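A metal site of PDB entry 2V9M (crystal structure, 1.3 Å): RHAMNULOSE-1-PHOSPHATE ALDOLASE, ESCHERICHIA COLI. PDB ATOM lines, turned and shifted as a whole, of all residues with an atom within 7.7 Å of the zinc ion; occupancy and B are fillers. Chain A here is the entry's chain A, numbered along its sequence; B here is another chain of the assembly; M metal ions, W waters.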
ATOM      1  N   TRP A  25       8.735   7.952 -11.661  1.00  0.00           N
ATOM      2  CA  TRP A  25       9.930   7.651 -10.847  1.00  0.00           C
ATOM      3  C   TRP A  25      10.978   6.877 -11.603  1.00  0.00           C
ATOM      4  O   TRP A  25      12.022   6.570 -11.012  1.00  0.00           O
ATOM      5  CB  TRP A  25       9.528   6.852  -9.622  1.00  0.00           C
ATOM      6  CG  TRP A  25       8.531   7.512  -8.696  1.00  0.00           C
ATOM      7  CD1 TRP A  25       8.167   8.813  -8.607  1.00  0.00           C
ATOM      8  CD2 TRP A  25       7.813   6.838  -7.646  1.00  0.00           C
ATOM      9  NE1 TRP A  25       7.236   8.989  -7.606  1.00  0.00           N
ATOM     10  CE2 TRP A  25       6.998   7.786  -7.000  1.00  0.00           C
ATOM     11  CE3 TRP A  25       7.753   5.499  -7.240  1.00  0.00           C
ATOM     12  CZ2 TRP A  25       6.156   7.458  -5.960  1.00  0.00           C
ATOM     13  CZ3 TRP A  25       6.911   5.172  -6.201  1.00  0.00           C
ATOM     14  CH2 TRP A  25       6.115   6.135  -5.555  1.00  0.00           C
ATOM     15  N   ASP A  26      10.709   6.419 -12.838  1.00  0.00           N
ATOM     16  CA  ASP A  26      11.556   5.404 -13.485  1.00  0.00           C
ATOM     17  C   ASP A  26      11.693   5.638 -14.984  1.00  0.00           C
ATOM     18  O   ASP A  26      11.373   4.809 -15.843  1.00  0.00           O
ATOM     19  CB  ASP A  26      11.070   3.991 -13.135  1.00  0.00           C
ATOM     20  CG  ASP A  26      11.242   3.680 -11.672  1.00  0.00           C
ATOM     21  OD1 ASP A  26      10.272   3.847 -10.911  1.00  0.00           O
ATOM     22  OD2 ASP A  26      12.403   3.353 -11.246  1.00  0.00           O
ATOM     23  N   GLU A  27      12.233   6.827 -15.296  1.00  0.00           N
ATOM     24  CA  GLU A  27      12.679   7.120 -16.654  1.00  0.00           C
ATOM     25  C   GLU A  27      13.681   6.080 -17.123  1.00  0.00           C
ATOM     26  O   GLU A  27      14.497   5.596 -16.324  1.00  0.00           O
ATOM     27  CB  GLU A  27      13.308   8.538 -16.695  1.00  0.00           C
ATOM     28  CG  GLU A  27      14.639   8.676 -15.942  1.00  0.00           C
ATOM     29  CD  GLU A  27      14.569   8.892 -14.446  1.00  0.00           C
ATOM     30  OE1 GLU A  27      15.665   9.134 -13.841  1.00  0.00           O
ATOM     31  OE2 GLU A  27      13.483   8.832 -13.850  1.00  0.00           O
ATOM     32  N   ARG A  28      13.659   5.797 -18.432  1.00  0.00           N
ATOM     33  CA  ARG A  28      14.708   4.971 -19.056  1.00  0.00           C
ATOM     34  C   ARG A  28      14.808   3.666 -18.294  1.00  0.00           C
ATOM     35  O   ARG A  28      13.759   3.041 -18.031  1.00  0.00           O
ATOM     36  CB  ARG A  28      15.978   5.828 -19.156  1.00  0.00           C
ATOM     37  CG  ARG A  28      17.000   5.355 -20.186  1.00  0.00           C
ATOM     38  CD  ARG A  28      18.372   6.008 -19.937  1.00  0.00           C
ATOM     39  NE  ARG A  28      18.965   5.596 -18.687  1.00  0.00           N
ATOM     40  CZ  ARG A  28      18.954   5.993 -17.446  1.00  0.00           C
ATOM     41  NH1 ARG A  28      18.340   7.033 -16.904  1.00  0.00           N
ATOM     42  NH2 ARG A  28      19.652   5.312 -16.496  1.00  0.00           N
ATOM     43  N   ASN A  29      16.020   3.247 -17.940  1.00  0.00           N
ATOM     44  CA  ASN A  29      16.270   2.052 -17.141  1.00  0.00           C
ATOM     45  C   ASN A  29      16.546   2.394 -15.679  1.00  0.00           C
ATOM     46  O   ASN A  29      17.114   1.592 -14.920  1.00  0.00           O
ATOM     47  CB  ASN A  29      17.436   1.276 -17.770  1.00  0.00           C
ATOM     48  CG  ASN A  29      18.730   2.046 -17.595  1.00  0.00           C
ATOM     49  OD1 ASN A  29      18.799   3.213 -17.840  1.00  0.00           O
ATOM     50  ND2 ASN A  29      19.801   1.390 -17.109  1.00  0.00           N
ATOM     51  N   GLY A  30      16.099   3.564 -15.210  1.00  0.00           N
ATOM     52  CA  GLY A  30      16.291   3.970 -13.834  1.00  0.00           C
ATOM     53  C   GLY A  30      15.434   3.194 -12.903  1.00  0.00           C
ATOM     54  O   GLY A  30      14.231   3.094 -13.074  1.00  0.00           O
ATOM     55  N   GLY A  31      15.971   2.510 -11.969  1.00  0.00           N
ATOM     56  CA  GLY A  31      15.268   1.764 -10.968  1.00  0.00           C
ATOM     57  C   GLY A  31      15.522   0.297 -11.077  1.00  0.00           C
ATOM     58  O   GLY A  31      15.971  -0.236 -12.105  1.00  0.00           O
ATOM     59  N   ASN A  32      15.304  -0.440 -10.004  1.00  0.00           N
ATOM     60  CA  ASN A  32      15.454  -1.860  -9.968  1.00  0.00           C
ATOM     61  C   ASN A  32      14.596  -2.379  -8.801  1.00  0.00           C
ATOM     62  O   ASN A  32      14.403  -1.703  -7.793  1.00  0.00           O
ATOM     63  CB  ASN A  32      16.900  -2.361  -9.707  1.00  0.00           C
ATOM     64  CG  ASN A  32      18.035  -1.684 -10.371  1.00  0.00           C
ATOM     65  OD1 ASN A  32      18.394  -0.525 -10.146  1.00  0.00           O
ATOM     66  ND2 ASN A  32      18.594  -2.356 -11.341  1.00  0.00           N
ATOM     67  N   GLU A 117      23.075  -5.832 -10.957  1.00  0.00           N
ATOM     68  CA  GLU A 117      22.794  -5.131  -9.702  1.00  0.00           C
ATOM     69  C   GLU A 117      22.378  -6.096  -8.601  1.00  0.00           C
ATOM     70  O   GLU A 117      22.168  -5.726  -7.436  1.00  0.00           O
ATOM     71  CB  GLU A 117      21.711  -4.073  -9.906  1.00  0.00           C
ATOM     72  CG  GLU A 117      22.175  -2.779 -10.569  1.00  0.00           C
ATOM     73  CD  GLU A 117      21.874  -2.649 -12.051  1.00  0.00           C
ATOM     74  OE1 GLU A 117      22.503  -3.469 -12.774  1.00  0.00           O
ATOM     75  OE2 GLU A 117      21.083  -1.799 -12.586  1.00  0.00           O
ATOM     76  N   HIS A 141      14.494   0.141  -5.694  1.00  0.00           N
ATOM     77  CA  HIS A 141      15.208   1.382  -6.001  1.00  0.00           C
ATOM     78  C   HIS A 141      14.424   2.126  -7.081  1.00  0.00           C
ATOM     79  O   HIS A 141      14.072   1.556  -8.124  1.00  0.00           O
ATOM     80  CB  HIS A 141      16.626   1.156  -6.463  1.00  0.00           C
ATOM     81  CG  HIS A 141      17.298   2.345  -7.070  1.00  0.00           C
ATOM     82  ND1 HIS A 141      17.453   3.546  -6.402  1.00  0.00           N
ATOM     83  CD2 HIS A 141      17.891   2.536  -8.261  1.00  0.00           C
ATOM     84  CE1 HIS A 141      18.087   4.401  -7.196  1.00  0.00           C
ATOM     85  NE2 HIS A 141      18.387   3.854  -8.331  1.00  0.00           N
ATOM     86  N   CYS A 142      14.141   3.418  -6.863  1.00  0.00           N
ATOM     87  CA  CYS A 142      13.562   4.224  -7.895  1.00  0.00           C
ATOM     88  C   CYS A 142      14.038   5.680  -7.771  1.00  0.00           C
ATOM     89  O   CYS A 142      14.683   6.039  -6.777  1.00  0.00           O
ATOM     90  CB  CYS A 142      12.053   4.128  -7.885  1.00  0.00           C
ATOM     91  SG  CYS A 142      11.327   4.824  -6.453  1.00  0.00           S
ATOM     92  N   HIS A 143      13.698   6.445  -8.781  1.00  0.00           N
ATOM     93  CA  HIS A 143      14.162   7.834  -8.860  1.00  0.00           C
ATOM     94  C   HIS A 143      12.976   8.744  -8.453  1.00  0.00           C
ATOM     95  O   HIS A 143      12.412   9.470  -9.265  1.00  0.00           O
ATOM     96  CB  HIS A 143      14.734   8.152 -10.232  1.00  0.00           C
ATOM     97  CG  HIS A 143      15.968   7.344 -10.524  1.00  0.00           C
ATOM     98  ND1 HIS A 143      16.584   7.406 -11.731  1.00  0.00           N
ATOM     99  CD2 HIS A 143      16.703   6.454  -9.795  1.00  0.00           C
ATOM    100  CE1 HIS A 143      17.654   6.601 -11.721  1.00  0.00           C
ATOM    101  NE2 HIS A 143      17.758   6.016 -10.533  1.00  0.00           N
ATOM    102  N   PRO A 188      27.453   5.229  -8.479  1.00  0.00           N
ATOM    103  CA  PRO A 188      26.585   4.067  -8.460  1.00  0.00           C
ATOM    104  C   PRO A 188      27.241   2.835  -9.085  1.00  0.00           C
ATOM    105  O   PRO A 188      28.178   2.889  -9.882  1.00  0.00           O
ATOM    106  CB  PRO A 188      25.376   4.448  -9.266  1.00  0.00           C
ATOM    107  CG  PRO A 188      25.580   5.812  -9.758  1.00  0.00           C
ATOM    108  CD  PRO A 188      26.969   6.249  -9.420  1.00  0.00           C
ATOM    109  N   TRP A 209      19.990   8.226  -1.669  1.00  0.00           N
ATOM    110  CA  TRP A 209      21.177   8.516  -2.439  1.00  0.00           C
ATOM    111  C   TRP A 209      21.048   9.940  -2.983  1.00  0.00           C
ATOM    112  O   TRP A 209      20.273  10.168  -3.912  1.00  0.00           O
ATOM    113  CB  TRP A 209      21.288   7.502  -3.577  1.00  0.00           C
ATOM    114  CG  TRP A 209      21.623   6.098  -3.177  1.00  0.00           C
ATOM    115  CD1 TRP A 209      21.895   5.591  -1.931  1.00  0.00           C
ATOM    116  CD2 TRP A 209      21.740   5.009  -4.093  1.00  0.00           C
ATOM    117  NE1 TRP A 209      22.162   4.255  -2.017  1.00  0.00           N
ATOM    118  CE2 TRP A 209      22.077   3.877  -3.342  1.00  0.00           C
ATOM    119  CE3 TRP A 209      21.601   4.878  -5.480  1.00  0.00           C
ATOM    120  CZ2 TRP A 209      22.282   2.638  -3.879  1.00  0.00           C
ATOM    121  CZ3 TRP A 209      21.805   3.642  -6.048  1.00  0.00           C
ATOM    122  CH2 TRP A 209      22.153   2.527  -5.266  1.00  0.00           C
ATOM    123  N   HIS A 212      20.138  11.408  -6.683  1.00  0.00           N
ATOM    124  CA  HIS A 212      19.954  10.137  -7.405  1.00  0.00           C
ATOM    125  C   HIS A 212      18.603   9.551  -7.034  1.00  0.00           C
ATOM    126  O   HIS A 212      17.801   9.363  -7.973  1.00  0.00           O
ATOM    127  CB  HIS A 212      21.138   9.198  -7.125  1.00  0.00           C
ATOM    128  CG  HIS A 212      21.083   7.895  -7.873  1.00  0.00           C
ATOM    129  ND1 HIS A 212      22.168   7.095  -8.066  1.00  0.00           N
ATOM    130  CD2 HIS A 212      20.104   7.190  -8.527  1.00  0.00           C
ATOM    131  CE1 HIS A 212      21.832   6.024  -8.743  1.00  0.00           C
ATOM    132  NE2 HIS A 212      20.547   6.039  -9.055  1.00  0.00           N
ATOM    133  N   GLY A 213      18.347   9.057  -5.857  1.00  0.00           N
ATOM    134  CA  GLY A 213      17.075   8.375  -5.632  1.00  0.00           C
ATOM    135  C   GLY A 213      16.978   7.696  -4.309  1.00  0.00           C
ATOM    136  O   GLY A 213      17.677   8.095  -3.355  1.00  0.00           O
ATOM    137  N   VAL A 214      16.078   6.726  -4.217  1.00  0.00           N
ATOM    138  CA  VAL A 214      15.703   6.103  -2.948  1.00  0.00           C
ATOM    139  C   VAL A 214      15.818   4.587  -3.056  1.00  0.00           C
ATOM    140  O   VAL A 214      15.689   4.038  -4.163  1.00  0.00           O
ATOM    141  CB  VAL A 214      14.291   6.557  -2.502  1.00  0.00           C
ATOM    142  CG1 VAL A 214      13.206   6.023  -3.431  1.00  0.00           C
ATOM    143  CG2 VAL A 214      13.980   6.169  -1.051  1.00  0.00           C
ATOM    144  N   THR B 170      21.877  11.933 -11.242  1.00  0.00           N
ATOM    145  CA  THR B 170      23.218  11.333 -11.344  1.00  0.00           C
ATOM    146  C   THR B 170      23.496  10.656 -12.667  1.00  0.00           C
ATOM    147  O   THR B 170      24.599  10.741 -13.206  1.00  0.00           O
ATOM    148  CB  THR B 170      23.423  10.358 -10.158  1.00  0.00           C
ATOM    149  OG1 THR B 170      23.627  11.105  -8.957  1.00  0.00           O
ATOM    150  CG2 THR B 170      24.650   9.484 -10.358  1.00  0.00           C
ATOM    151  N   GLU B 171      22.496   9.967 -13.230  1.00  0.00           N
ATOM    152  CA  GLU B 171      22.562   9.222 -14.484  1.00  0.00           C
ATOM    153  C   GLU B 171      22.896  10.083 -15.684  1.00  0.00           C
ATOM    154  O   GLU B 171      23.378   9.570 -16.688  1.00  0.00           O
ATOM    155  CB  GLU B 171      21.209   8.526 -14.792  1.00  0.00           C
ATOM    156  CG  GLU B 171      20.094   9.542 -14.952  1.00  0.00           C
ATOM    157  CD  GLU B 171      18.684   9.073 -14.728  1.00  0.00           C
ATOM    158  OE1 GLU B 171      18.413   7.895 -14.587  1.00  0.00           O
ATOM    159  OE2 GLU B 171      17.791   9.885 -14.674  1.00  0.00           O
HETATM  160 ZN    ZN M   1      19.273   4.772  -9.931  1.00  0.00          ZN
HETATM  161  O   HOH W   1      21.182   3.306  -9.944  1.00  0.00           O
HETATM  162  O   HOH W   2      19.125   3.232 -11.402  1.00  0.00           O
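The zinc ion is bound by a ring nitrogen (NE2) of His 212 (2.0 Å), a ring nitrogen (NE2) of His 141 (2.0 Å), a ring nitrogen (NE2) of His 143 (2.1 Å), water W2 (2.1 Å) and water W1 (2.4 Å).
The backbone carbonyl oxygen of Asn 32 is in hydrogen-bond range of the backbone NH of His 141, 2.8 Å away. ND1 of His 141 lies within hydrogen-bond range of O of Val 214, at 2.9 Å. A ring nitrogen (ND1) of His 143 lies close to the side-chain carboxylate of Glu 171 of chain B. A ring nitrogen (ND1) of His 143 is in hydrogen-bond range of the side-chain carboxylate (OE1) of Glu 27 (2.9 Å). The backbone NH of His 143 sits at hydrogen-bond distance from the backbone carbonyl oxygen of Trp 25 (2.8 Å).
Of the 19 residues printed, 3 come within 4 Å of the zinc ion. The nearest printed residue that does not touch the zinc ion is Gly 31 (4.5 Å).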
